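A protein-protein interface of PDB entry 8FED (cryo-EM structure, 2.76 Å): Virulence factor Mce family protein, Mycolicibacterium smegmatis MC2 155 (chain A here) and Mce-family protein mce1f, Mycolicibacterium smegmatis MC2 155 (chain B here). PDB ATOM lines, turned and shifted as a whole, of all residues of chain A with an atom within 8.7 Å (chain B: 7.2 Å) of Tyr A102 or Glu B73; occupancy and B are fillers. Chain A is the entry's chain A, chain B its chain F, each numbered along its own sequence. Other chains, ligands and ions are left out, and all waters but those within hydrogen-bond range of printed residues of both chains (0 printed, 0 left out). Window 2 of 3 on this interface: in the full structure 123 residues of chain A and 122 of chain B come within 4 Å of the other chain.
Of the printed residues of chain B, Gly A72 touches Ser B50 (3.4 Å). Of chain B, only Glu B73 (3.8 Å) and Pro B74 (3.4 Å) come within 4 Å of Tyr A102. Of the printed residues of chain B, Leu A105 touches Pro B74, Ser B75 and Glu B76. Glu B73 touches just one residue of chain A: Tyr A102. Printed residues of chain A within 4 Å of Pro B74: Val A73, Tyr A102 and Leu A105. Of the printed residues of chain A, Ser B75 touches Phe A70 (3.9 Å), Asn A71 (2.9 Å) and Leu A105 (3.9 Å). Of the printed residues of chain A, Glu B76 touches Leu A105 (3.9 Å). Printed residues of chain A within 4 Å of Gly B78: Asn A71 (3.0 Å). The nearest residue of chain A that does not touch Glu B73 is Val A73 (4.3 Å). The nearest printed residue of chain B that does not touch Gly A72 is Ala B79 (6.4 Å).
The backbone carbonyl oxygen (O) of Asn A71 lies within hydrogen-bond range of the backbone NH (N) of Ser B50, at 2.8 Å. The backbone carbonyl oxygen of Ser B75 sits at hydrogen-bond distance from the side-chain amide nitrogen of Asn A71, 2.9 Å away. The backbone carbonyl oxygen (O) of Gly B78 sits at hydrogen-bond distance from the side-chain amide nitrogen (ND2) of Asn A71 (3.0 Å).
Of the 12 printed residues of chain B, 7 touch a printed residue of chain A. Of the 25 printed residues of chain A, 6 touch a printed residue of chain B. Printed residues of chain A that touch a printed residue of chain B: Phe A70, Asn A71, Gly A72, Val A73, Tyr A102 and Leu A105. Hydrophobic or aromatic side chains of chain A that line the printed part of chain B: Phe A70, Val A73, Tyr A102 and Leu A105. Among the printed residues, 13 pairs touch across the chains.
O of Gly B78 sits at hydrogen-bond distance from OG of Ser B75 (3.0 Å). N of Ala B79 is in hydrogen-bond range of OG of Ser B75 (3.4 Å). The backbone carbonyl oxygen (O) of Leu A105 sits at hydrogen-bond distance from the guanidinium group (NH2) of Arg A137, at 3.2 Å. NZ of Lys A101 is in hydrogen-bond range of OH of Tyr A102, at 3.5 Å. O of Glu B73 is in hydrogen-bond range of N of Arg B80 (2.9 Å).
Phe A70 touches Ser B75. Ser B50 touches Gly A72. CB of Ser B50 touches CG1 of Val A73 (3.5 Å). CG1 of Val A73 touches CG1 of Val B72, at 3.6 Å. Pro B74 touches Val A73 (CD to CG2, 3.5 Å). Glu B73 touches Tyr A102. Tyr A102 touches Pro B74 (CD1 to CG, 3.4 Å). Leu A105 touches Pro B74. Leu A105 touches Ser B75 (CD2 to O, 3.9 Å). N of Glu B76 touches CD1 of Leu A105, 3.9 Å away.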
ATOM      1  N   LYS A  48      -2.682 -11.259 -27.103  1.00  0.00           N
ATOM      2  CA  LYS A  48      -2.583 -12.565 -26.472  1.00  0.00           C
ATOM      3  C   LYS A  48      -1.155 -13.073 -26.619  1.00  0.00           C
ATOM      4  O   LYS A  48      -0.361 -12.541 -27.399  1.00  0.00           O
ATOM      5  CB  LYS A  48      -3.575 -13.565 -27.082  1.00  0.00           C
ATOM      6  CG  LYS A  48      -5.032 -13.251 -26.795  1.00  0.00           C
ATOM      7  CD  LYS A  48      -5.941 -14.346 -27.327  1.00  0.00           C
ATOM      8  CE  LYS A  48      -7.367 -14.171 -26.836  1.00  0.00           C
ATOM      9  NZ  LYS A  48      -8.230 -15.317 -27.236  1.00  0.00           N
ATOM     10  N   VAL A  49      -0.828 -14.114 -25.859  1.00  0.00           N
ATOM     11  CA  VAL A  49       0.511 -14.692 -25.856  1.00  0.00           C
ATOM     12  C   VAL A  49       0.452 -16.064 -26.514  1.00  0.00           C
ATOM     13  O   VAL A  49      -0.508 -16.820 -26.317  1.00  0.00           O
ATOM     14  CB  VAL A  49       1.088 -14.762 -24.425  1.00  0.00           C
ATOM     15  CG1 VAL A  49       0.077 -15.348 -23.463  1.00  0.00           C
ATOM     16  CG2 VAL A  49       2.397 -15.543 -24.387  1.00  0.00           C
ATOM     17  N   LEU A  51       1.719 -19.823 -27.080  1.00  0.00           N
ATOM     18  CA  LEU A  51       2.364 -20.950 -26.425  1.00  0.00           C
ATOM     19  C   LEU A  51       2.525 -22.089 -27.420  1.00  0.00           C
ATOM     20  O   LEU A  51       1.618 -22.368 -28.211  1.00  0.00           O
ATOM     21  CB  LEU A  51       1.564 -21.434 -25.212  1.00  0.00           C
ATOM     22  CG  LEU A  51       1.108 -20.392 -24.193  1.00  0.00           C
ATOM     23  CD1 LEU A  51       0.376 -21.067 -23.048  1.00  0.00           C
ATOM     24  CD2 LEU A  51       2.289 -19.592 -23.674  1.00  0.00           C
ATOM     25  N   VAL A  68      -9.082 -23.789 -25.863  1.00  0.00           N
ATOM     26  CA  VAL A  68      -8.070 -24.216 -24.906  1.00  0.00           C
ATOM     27  C   VAL A  68      -8.616 -23.896 -23.525  1.00  0.00           C
ATOM     28  O   VAL A  68      -8.749 -22.723 -23.164  1.00  0.00           O
ATOM     29  CB  VAL A  68      -6.728 -23.514 -25.143  1.00  0.00           C
ATOM     30  CG1 VAL A  68      -5.747 -23.868 -24.045  1.00  0.00           C
ATOM     31  CG2 VAL A  68      -6.174 -23.876 -26.503  1.00  0.00           C
ATOM     32  N   THR A  69      -8.935 -24.925 -22.749  1.00  0.00           N
ATOM     33  CA  THR A  69      -9.612 -24.749 -21.471  1.00  0.00           C
ATOM     34  C   THR A  69      -8.680 -25.115 -20.326  1.00  0.00           C
ATOM     35  O   THR A  69      -8.010 -26.151 -20.370  1.00  0.00           O
ATOM     36  CB  THR A  69     -10.877 -25.603 -21.395  1.00  0.00           C
ATOM     37  OG1 THR A  69     -10.517 -26.970 -21.170  1.00  0.00           O
ATOM     38  CG2 THR A  69     -11.667 -25.505 -22.688  1.00  0.00           C
ATOM     39  N   PHE A  70      -8.647 -24.266 -19.306  1.00  0.00           N
ATOM     40  CA  PHE A  70      -7.985 -24.562 -18.046  1.00  0.00           C
ATOM     41  C   PHE A  70      -9.064 -24.844 -17.011  1.00  0.00           C
ATOM     42  O   PHE A  70     -10.036 -24.088 -16.912  1.00  0.00           O
ATOM     43  CB  PHE A  70      -7.093 -23.403 -17.599  1.00  0.00           C
ATOM     44  CG  PHE A  70      -6.402 -23.636 -16.286  1.00  0.00           C
ATOM     45  CD1 PHE A  70      -5.285 -24.449 -16.210  1.00  0.00           C
ATOM     46  CD2 PHE A  70      -6.864 -23.034 -15.130  1.00  0.00           C
ATOM     47  CE1 PHE A  70      -4.648 -24.664 -15.004  1.00  0.00           C
ATOM     48  CE2 PHE A  70      -6.229 -23.245 -13.922  1.00  0.00           C
ATOM     49  CZ  PHE A  70      -5.120 -24.061 -13.861  1.00  0.00           C
ATOM     50  N   ASN A  71      -8.922 -25.954 -16.287  1.00  0.00           N
ATOM     51  CA  ASN A  71      -9.890 -26.391 -15.280  1.00  0.00           C
ATOM     52  C   ASN A  71     -11.305 -26.523 -15.842  1.00  0.00           C
ATOM     53  O   ASN A  71     -12.274 -26.579 -15.081  1.00  0.00           O
ATOM     54  CB  ASN A  71      -9.895 -25.460 -14.061  1.00  0.00           C
ATOM     55  CG  ASN A  71      -8.794 -25.787 -13.075  1.00  0.00           C
ATOM     56  OD1 ASN A  71      -8.245 -26.887 -13.084  1.00  0.00           O
ATOM     57  ND2 ASN A  71      -8.476 -24.834 -12.209  1.00  0.00           N
ATOM     58  N   GLY A  72     -11.444 -26.582 -17.165  1.00  0.00           N
ATOM     59  CA  GLY A  72     -12.732 -26.725 -17.804  1.00  0.00           C
ATOM     60  C   GLY A  72     -13.328 -25.452 -18.366  1.00  0.00           C
ATOM     61  O   GLY A  72     -14.389 -25.520 -18.998  1.00  0.00           O
ATOM     62  N   VAL A  73     -12.700 -24.303 -18.162  1.00  0.00           N
ATOM     63  CA  VAL A  73     -13.197 -23.025 -18.668  1.00  0.00           C
ATOM     64  C   VAL A  73     -12.224 -22.504 -19.716  1.00  0.00           C
ATOM     65  O   VAL A  73     -11.007 -22.606 -19.519  1.00  0.00           O
ATOM     66  CB  VAL A  73     -13.401 -21.986 -17.547  1.00  0.00           C
ATOM     67  CG1 VAL A  73     -14.467 -22.439 -16.597  1.00  0.00           C
ATOM     68  CG2 VAL A  73     -12.134 -21.772 -16.779  1.00  0.00           C
ATOM     69  N   PRO A  74     -12.705 -22.016 -20.858  1.00  0.00           N
ATOM     70  CA  PRO A  74     -11.792 -21.549 -21.905  1.00  0.00           C
ATOM     71  C   PRO A  74     -10.954 -20.373 -21.430  1.00  0.00           C
ATOM     72  O   PRO A  74     -11.399 -19.541 -20.636  1.00  0.00           O
ATOM     73  CB  PRO A  74     -12.736 -21.142 -23.042  1.00  0.00           C
ATOM     74  CG  PRO A  74     -13.980 -21.924 -22.792  1.00  0.00           C
ATOM     75  CD  PRO A  74     -14.107 -22.008 -21.305  1.00  0.00           C
ATOM     76  N   ILE A  75      -9.721 -20.317 -21.927  1.00  0.00           N
ATOM     77  CA  ILE A  75      -8.778 -19.255 -21.606  1.00  0.00           C
ATOM     78  C   ILE A  75      -8.202 -18.726 -22.910  1.00  0.00           C
ATOM     79  O   ILE A  75      -7.557 -17.673 -22.941  1.00  0.00           O
ATOM     80  CB  ILE A  75      -7.658 -19.756 -20.677  1.00  0.00           C
ATOM     81  CG1 ILE A  75      -6.814 -20.805 -21.399  1.00  0.00           C
ATOM     82  CG2 ILE A  75      -8.233 -20.306 -19.381  1.00  0.00           C
ATOM     83  CD1 ILE A  75      -5.762 -21.440 -20.545  1.00  0.00           C
ATOM     84  N   GLY A  76      -8.430 -19.456 -23.989  1.00  0.00           N
ATOM     85  CA  GLY A  76      -7.885 -19.074 -25.270  1.00  0.00           C
ATOM     86  C   GLY A  76      -8.435 -19.946 -26.372  1.00  0.00           C
ATOM     87  O   GLY A  76      -9.466 -20.602 -26.213  1.00  0.00           O
ATOM     88  N   ASP A  97      -2.990 -19.213 -28.967  1.00  0.00           N
ATOM     89  CA  ASP A  97      -3.114 -17.815 -28.563  1.00  0.00           C
ATOM     90  C   ASP A  97      -3.984 -17.757 -27.313  1.00  0.00           C
ATOM     91  O   ASP A  97      -5.186 -18.032 -27.375  1.00  0.00           O
ATOM     92  CB  ASP A  97      -3.706 -16.973 -29.689  1.00  0.00           C
ATOM     93  CG  ASP A  97      -2.847 -16.979 -30.933  1.00  0.00           C
ATOM     94  OD1 ASP A  97      -1.769 -17.607 -30.907  1.00  0.00           O
ATOM     95  OD2 ASP A  97      -3.249 -16.355 -31.938  1.00  0.00           O
ATOM     96  N   VAL A  98      -3.382 -17.407 -26.176  1.00  0.00           N
ATOM     97  CA  VAL A  98      -4.060 -17.459 -24.886  1.00  0.00           C
ATOM     98  C   VAL A  98      -4.014 -16.076 -24.249  1.00  0.00           C
ATOM     99  O   VAL A  98      -3.012 -15.359 -24.363  1.00  0.00           O
ATOM    100  CB  VAL A  98      -3.442 -18.534 -23.964  1.00  0.00           C
ATOM    101  CG1 VAL A  98      -1.953 -18.328 -23.814  1.00  0.00           C
ATOM    102  CG2 VAL A  98      -4.128 -18.564 -22.605  1.00  0.00           C
ATOM    103  N   ASP A  99      -5.122 -15.690 -23.620  1.00  0.00           N
ATOM    104  CA  ASP A  99      -5.211 -14.402 -22.937  1.00  0.00           C
ATOM    105  C   ASP A  99      -4.263 -14.380 -21.742  1.00  0.00           C
ATOM    106  O   ASP A  99      -4.300 -15.294 -20.911  1.00  0.00           O
ATOM    107  CB  ASP A  99      -6.656 -14.172 -22.485  1.00  0.00           C
ATOM    108  CG  ASP A  99      -6.966 -12.713 -22.198  1.00  0.00           C
ATOM    109  OD1 ASP A  99      -6.139 -12.024 -21.572  1.00  0.00           O
ATOM    110  OD2 ASP A  99      -8.053 -12.253 -22.605  1.00  0.00           O
ATOM    111  N   PRO A 100      -3.408 -13.359 -21.613  1.00  0.00           N
ATOM    112  CA  PRO A 100      -2.443 -13.325 -20.501  1.00  0.00           C
ATOM    113  C   PRO A 100      -3.057 -13.118 -19.123  1.00  0.00           C
ATOM    114  O   PRO A 100      -2.311 -13.127 -18.137  1.00  0.00           O
ATOM    115  CB  PRO A 100      -1.527 -12.149 -20.873  1.00  0.00           C
ATOM    116  CG  PRO A 100      -2.345 -11.302 -21.782  1.00  0.00           C
ATOM    117  CD  PRO A 100      -3.183 -12.260 -22.568  1.00  0.00           C
ATOM    118  N   LYS A 101      -4.373 -12.917 -19.015  1.00  0.00           N
ATOM    119  CA  LYS A 101      -4.996 -12.769 -17.700  1.00  0.00           C
ATOM    120  C   LYS A 101      -4.840 -14.034 -16.867  1.00  0.00           C
ATOM    121  O   LYS A 101      -4.554 -13.966 -15.665  1.00  0.00           O
ATOM    122  CB  LYS A 101      -6.474 -12.412 -17.848  1.00  0.00           C
ATOM    123  CG  LYS A 101      -6.741 -11.115 -18.586  1.00  0.00           C
ATOM    124  CD  LYS A 101      -8.220 -10.766 -18.558  1.00  0.00           C
ATOM    125  CE  LYS A 101      -9.071 -11.924 -19.055  1.00  0.00           C
ATOM    126  NZ  LYS A 101     -10.527 -11.632 -18.949  1.00  0.00           N
ATOM    127  N   TYR A 102      -5.028 -15.196 -17.483  1.00  0.00           N
ATOM    128  CA  TYR A 102      -4.955 -16.476 -16.794  1.00  0.00           C
ATOM    129  C   TYR A 102      -3.559 -17.083 -16.812  1.00  0.00           C
ATOM    130  O   TYR A 102      -3.363 -18.157 -16.234  1.00  0.00           O
ATOM    131  CB  TYR A 102      -5.946 -17.461 -17.418  1.00  0.00           C
ATOM    132  CG  TYR A 102      -7.231 -16.822 -17.890  1.00  0.00           C
ATOM    133  CD1 TYR A 102      -8.257 -16.546 -17.002  1.00  0.00           C
ATOM    134  CD2 TYR A 102      -7.421 -16.507 -19.228  1.00  0.00           C
ATOM    135  CE1 TYR A 102      -9.437 -15.971 -17.427  1.00  0.00           C
ATOM    136  CE2 TYR A 102      -8.597 -15.931 -19.665  1.00  0.00           C
ATOM    137  CZ  TYR A 102      -9.601 -15.666 -18.759  1.00  0.00           C
ATOM    138  OH  TYR A 102     -10.775 -15.089 -19.186  1.00  0.00           O
ATOM    139  N   LEU A 103      -2.595 -16.429 -17.464  1.00  0.00           N
ATOM    140  CA  LEU A 103      -1.249 -16.987 -17.571  1.00  0.00           C
ATOM    141  C   LEU A 103      -0.584 -17.110 -16.206  1.00  0.00           C
ATOM    142  O   LEU A 103       0.124 -18.087 -15.937  1.00  0.00           O
ATOM    143  CB  LEU A 103      -0.398 -16.123 -18.500  1.00  0.00           C
ATOM    144  CG  LEU A 103       0.532 -16.883 -19.445  1.00  0.00           C
ATOM    145  CD1 LEU A 103      -0.281 -17.664 -20.462  1.00  0.00           C
ATOM    146  CD2 LEU A 103       1.505 -15.938 -20.128  1.00  0.00           C
ATOM    147  N   ASP A 104      -0.794 -16.126 -15.330  1.00  0.00           N
ATOM    148  CA  ASP A 104      -0.223 -16.163 -13.989  1.00  0.00           C
ATOM    149  C   ASP A 104      -0.872 -17.218 -13.098  1.00  0.00           C
ATOM    150  O   ASP A 104      -0.340 -17.506 -12.020  1.00  0.00           O
ATOM    151  CB  ASP A 104      -0.342 -14.781 -13.340  1.00  0.00           C
ATOM    152  CG  ASP A 104       0.514 -14.641 -12.097  1.00  0.00           C
ATOM    153  OD1 ASP A 104       1.755 -14.604 -12.229  1.00  0.00           O
ATOM    154  OD2 ASP A 104      -0.054 -14.569 -10.988  1.00  0.00           O
ATOM    155  N   LEU A 105      -1.988 -17.806 -13.521  1.00  0.00           N
ATOM    156  CA  LEU A 105      -2.683 -18.807 -12.723  1.00  0.00           C
ATOM    157  C   LEU A 105      -2.255 -20.233 -13.049  1.00  0.00           C
ATOM    158  O   LEU A 105      -2.261 -21.092 -12.160  1.00  0.00           O
ATOM    159  CB  LEU A 105      -4.196 -18.667 -12.921  1.00  0.00           C
ATOM    160  CG  LEU A 105      -5.122 -19.604 -12.144  1.00  0.00           C
ATOM    161  CD1 LEU A 105      -4.952 -19.405 -10.650  1.00  0.00           C
ATOM    162  CD2 LEU A 105      -6.566 -19.380 -12.557  1.00  0.00           C
ATOM    163  N   ILE A 106      -1.873 -20.500 -14.290  1.00  0.00           N
ATOM    164  CA  ILE A 106      -1.545 -21.864 -14.711  1.00  0.00           C
ATOM    165  C   ILE A 106      -0.115 -22.187 -14.285  1.00  0.00           C
ATOM    166  O   ILE A 106       0.809 -21.433 -14.624  1.00  0.00           O
ATOM    167  CB  ILE A 106      -1.709 -22.011 -16.216  1.00  0.00           C
ATOM    168  CG1 ILE A 106      -3.017 -21.370 -16.671  1.00  0.00           C
ATOM    169  CG2 ILE A 106      -1.696 -23.474 -16.608  1.00  0.00           C
ATOM    170  CD1 ILE A 106      -3.109 -21.216 -18.158  1.00  0.00           C
ATOM    171  N   PRO A 107       0.106 -23.281 -13.560  1.00  0.00           N
ATOM    172  CA  PRO A 107       1.469 -23.645 -13.165  1.00  0.00           C
ATOM    173  C   PRO A 107       2.293 -24.124 -14.350  1.00  0.00           C
ATOM    174  O   PRO A 107       1.771 -24.490 -15.405  1.00  0.00           O
ATOM    175  CB  PRO A 107       1.254 -24.772 -12.152  1.00  0.00           C
ATOM    176  CG  PRO A 107      -0.049 -25.372 -12.541  1.00  0.00           C
ATOM    177  CD  PRO A 107      -0.893 -24.236 -13.049  1.00  0.00           C
ATOM    178  N   ARG A 137       5.661 -19.868 -13.622  1.00  0.00           N
ATOM    179  CA  ARG A 137       4.478 -19.782 -14.463  1.00  0.00           C
ATOM    180  C   ARG A 137       4.860 -19.929 -15.930  1.00  0.00           C
ATOM    181  O   ARG A 137       5.944 -19.511 -16.351  1.00  0.00           O
ATOM    182  CB  ARG A 137       3.743 -18.456 -14.243  1.00  0.00           C
ATOM    183  CG  ARG A 137       2.479 -18.585 -13.413  1.00  0.00           C
ATOM    184  CD  ARG A 137       2.710 -19.419 -12.167  1.00  0.00           C
ATOM    185  NE  ARG A 137       1.459 -19.767 -11.507  1.00  0.00           N
ATOM    186  CZ  ARG A 137       1.353 -20.660 -10.533  1.00  0.00           C
ATOM    187  NH1 ARG A 137       2.408 -21.318 -10.082  1.00  0.00           N
ATOM    188  NH2 ARG A 137       0.158 -20.906 -10.005  1.00  0.00           N
ATOM    189  N   LEU A 138       3.964 -20.538 -16.703  1.00  0.00           N
ATOM    190  CA  LEU A 138       4.234 -20.777 -18.113  1.00  0.00           C
ATOM    191  C   LEU A 138       4.261 -19.469 -18.899  1.00  0.00           C
ATOM    192  O   LEU A 138       3.630 -18.477 -18.527  1.00  0.00           O
ATOM    193  CB  LEU A 138       3.200 -21.733 -18.713  1.00  0.00           C
ATOM    194  CG  LEU A 138       1.751 -21.780 -18.221  1.00  0.00           C
ATOM    195  CD1 LEU A 138       1.039 -20.449 -18.372  1.00  0.00           C
ATOM    196  CD2 LEU A 138       1.003 -22.862 -18.981  1.00  0.00           C
ATOM    197  N   SER B  50     -14.898 -27.244 -14.296  1.00  0.00           N
ATOM    198  CA  SER B  50     -16.093 -26.588 -14.813  1.00  0.00           C
ATOM    199  C   SER B  50     -17.110 -27.593 -15.330  1.00  0.00           C
ATOM    200  O   SER B  50     -18.322 -27.391 -15.189  1.00  0.00           O
ATOM    201  CB  SER B  50     -15.719 -25.614 -15.920  1.00  0.00           C
ATOM    202  OG  SER B  50     -16.876 -25.042 -16.504  1.00  0.00           O
ATOM    203  N   SER B  71     -21.620 -16.036 -14.409  1.00  0.00           N
ATOM    204  CA  SER B  71     -20.233 -16.098 -14.849  1.00  0.00           C
ATOM    205  C   SER B  71     -19.575 -17.365 -14.327  1.00  0.00           C
ATOM    206  O   SER B  71     -19.924 -17.869 -13.259  1.00  0.00           O
ATOM    207  CB  SER B  71     -19.444 -14.870 -14.385  1.00  0.00           C
ATOM    208  OG  SER B  71     -19.321 -14.847 -12.974  1.00  0.00           O
ATOM    209  N   VAL B  72     -18.625 -17.878 -15.107  1.00  0.00           N
ATOM    210  CA  VAL B  72     -17.769 -18.989 -14.708  1.00  0.00           C
ATOM    211  C   VAL B  72     -16.326 -18.560 -14.931  1.00  0.00           C
ATOM    212  O   VAL B  72     -15.976 -18.097 -16.022  1.00  0.00           O
ATOM    213  CB  VAL B  72     -18.075 -20.278 -15.496  1.00  0.00           C
ATOM    214  CG1 VAL B  72     -17.448 -21.471 -14.809  1.00  0.00           C
ATOM    215  CG2 VAL B  72     -19.572 -20.484 -15.646  1.00  0.00           C
ATOM    216  N   GLU B  73     -15.494 -18.711 -13.905  1.00  0.00           N
ATOM    217  CA  GLU B  73     -14.127 -18.220 -13.949  1.00  0.00           C
ATOM    218  C   GLU B  73     -13.162 -19.293 -13.466  1.00  0.00           C
ATOM    219  O   GLU B  73     -13.508 -20.101 -12.600  1.00  0.00           O
ATOM    220  CB  GLU B  73     -13.982 -16.963 -13.075  1.00  0.00           C
ATOM    221  CG  GLU B  73     -12.992 -15.930 -13.586  1.00  0.00           C
ATOM    222  CD  GLU B  73     -13.451 -15.265 -14.869  1.00  0.00           C
ATOM    223  OE1 GLU B  73     -14.675 -15.218 -15.113  1.00  0.00           O
ATOM    224  OE2 GLU B  73     -12.587 -14.791 -15.635  1.00  0.00           O
ATOM    225  N   PRO B  74     -11.952 -19.338 -14.021  1.00  0.00           N
ATOM    226  CA  PRO B  74     -10.936 -20.254 -13.490  1.00  0.00           C
ATOM    227  C   PRO B  74     -10.417 -19.804 -12.135  1.00  0.00           C
ATOM    228  O   PRO B  74     -10.315 -18.610 -11.844  1.00  0.00           O
ATOM    229  CB  PRO B  74      -9.825 -20.205 -14.545  1.00  0.00           C
ATOM    230  CG  PRO B  74     -10.015 -18.908 -15.220  1.00  0.00           C
ATOM    231  CD  PRO B  74     -11.487 -18.655 -15.238  1.00  0.00           C
ATOM    232  N   SER B  75     -10.078 -20.786 -11.304  1.00  0.00           N
ATOM    233  CA  SER B  75      -9.505 -20.532  -9.993  1.00  0.00           C
ATOM    234  C   SER B  75      -8.366 -21.514  -9.764  1.00  0.00           C
ATOM    235  O   SER B  75      -8.115 -22.408 -10.575  1.00  0.00           O
ATOM    236  CB  SER B  75     -10.555 -20.643  -8.881  1.00  0.00           C
ATOM    237  OG  SER B  75     -11.069 -21.958  -8.790  1.00  0.00           O
ATOM    238  N   GLU B  76      -7.666 -21.335  -8.642  1.00  0.00           N
ATOM    239  CA  GLU B  76      -6.545 -22.214  -8.329  1.00  0.00           C
ATOM    240  C   GLU B  76      -7.009 -23.620  -7.967  1.00  0.00           C
ATOM    241  O   GLU B  76      -6.328 -24.598  -8.296  1.00  0.00           O
ATOM    242  CB  GLU B  76      -5.696 -21.616  -7.199  1.00  0.00           C
ATOM    243  CG  GLU B  76      -6.397 -21.451  -5.849  1.00  0.00           C
ATOM    244  CD  GLU B  76      -7.360 -20.276  -5.808  1.00  0.00           C
ATOM    245  OE1 GLU B  76      -7.324 -19.440  -6.736  1.00  0.00           O
ATOM    246  OE2 GLU B  76      -8.153 -20.191  -4.847  1.00  0.00           O
ATOM    247  N   GLY B  78      -9.993 -25.022  -8.895  1.00  0.00           N
ATOM    248  CA  GLY B  78     -11.056 -25.490  -9.760  1.00  0.00           C
ATOM    249  C   GLY B  78     -11.698 -24.373 -10.553  1.00  0.00           C
ATOM    250  O   GLY B  78     -11.011 -23.635 -11.264  1.00  0.00           O
ATOM    251  N   ALA B  79     -13.016 -24.241 -10.444  1.00  0.00           N
ATOM    252  CA  ALA B  79     -13.756 -23.188 -11.121  1.00  0.00           C
ATOM    253  C   ALA B  79     -14.698 -22.513 -10.136  1.00  0.00           C
ATOM    254  O   ALA B  79     -15.227 -23.147  -9.220  1.00  0.00           O
ATOM    255  CB  ALA B  79     -14.547 -23.734 -12.315  1.00  0.00           C
ATOM    256  N   ARG B  80     -14.901 -21.214 -10.333  1.00  0.00           N
ATOM    257  CA  ARG B  80     -15.796 -20.412  -9.512  1.00  0.00           C
ATOM    258  C   ARG B  80     -16.991 -19.997 -10.359  1.00  0.00           C
ATOM    259  O   ARG B  80     -16.821 -19.397 -11.425  1.00  0.00           O
ATOM    260  CB  ARG B  80     -15.064 -19.186  -8.966  1.00  0.00           C
ATOM    261  CG  ARG B  80     -15.954 -18.152  -8.308  1.00  0.00           C
ATOM    262  CD  ARG B  80     -16.543 -18.668  -7.012  1.00  0.00           C
ATOM    263  NE  ARG B  80     -17.316 -17.639  -6.330  1.00  0.00           N
ATOM    264  CZ  ARG B  80     -16.789 -16.703  -5.554  1.00  0.00           C
ATOM    265  NH1 ARG B  80     -15.486 -16.636  -5.338  1.00  0.00           N
ATOM    266  NH2 ARG B  80     -17.589 -15.808  -4.982  1.00  0.00           N
ATOM    267  N   VAL B  81     -18.192 -20.310  -9.884  1.00  0.00           N
ATOM    268  CA  VAL B  81     -19.427 -20.048 -10.611  1.00  0.00           C
ATOM    269  C   VAL B  81     -20.246 -19.044  -9.817  1.00  0.00           C
ATOM    270  O   VAL B  81     -20.482 -19.240  -8.619  1.00  0.00           O
ATOM    271  CB  VAL B  81     -20.225 -21.343 -10.849  1.00  0.00           C
ATOM    272  CG1 VAL B  81     -21.614 -21.027 -11.374  1.00  0.00           C
ATOM    273  CG2 VAL B  81     -19.488 -22.240 -11.815  1.00  0.00           C
ATOM    274  N   GLU B  82     -20.667 -17.972 -10.476  1.00  0.00           N
ATOM    275  CA  GLU B  82     -21.581 -16.994  -9.907  1.00  0.00           C
ATOM    276  C   GLU B  82     -22.877 -17.039 -10.700  1.00  0.00           C
ATOM    277  O   GLU B  82     -22.852 -17.006 -11.935  1.00  0.00           O
ATOM    278  CB  GLU B  82     -20.978 -15.589  -9.946  1.00  0.00           C
ATOM    279  CG  GLU B  82     -19.590 -15.499  -9.339  1.00  0.00           C
ATOM    280  CD  GLU B  82     -18.893 -14.194  -9.666  1.00  0.00           C
ATOM    281  OE1 GLU B  82     -19.490 -13.362 -10.381  1.00  0.00           O
ATOM    282  OE2 GLU B  82     -17.746 -14.000  -9.210  1.00  0.00           O
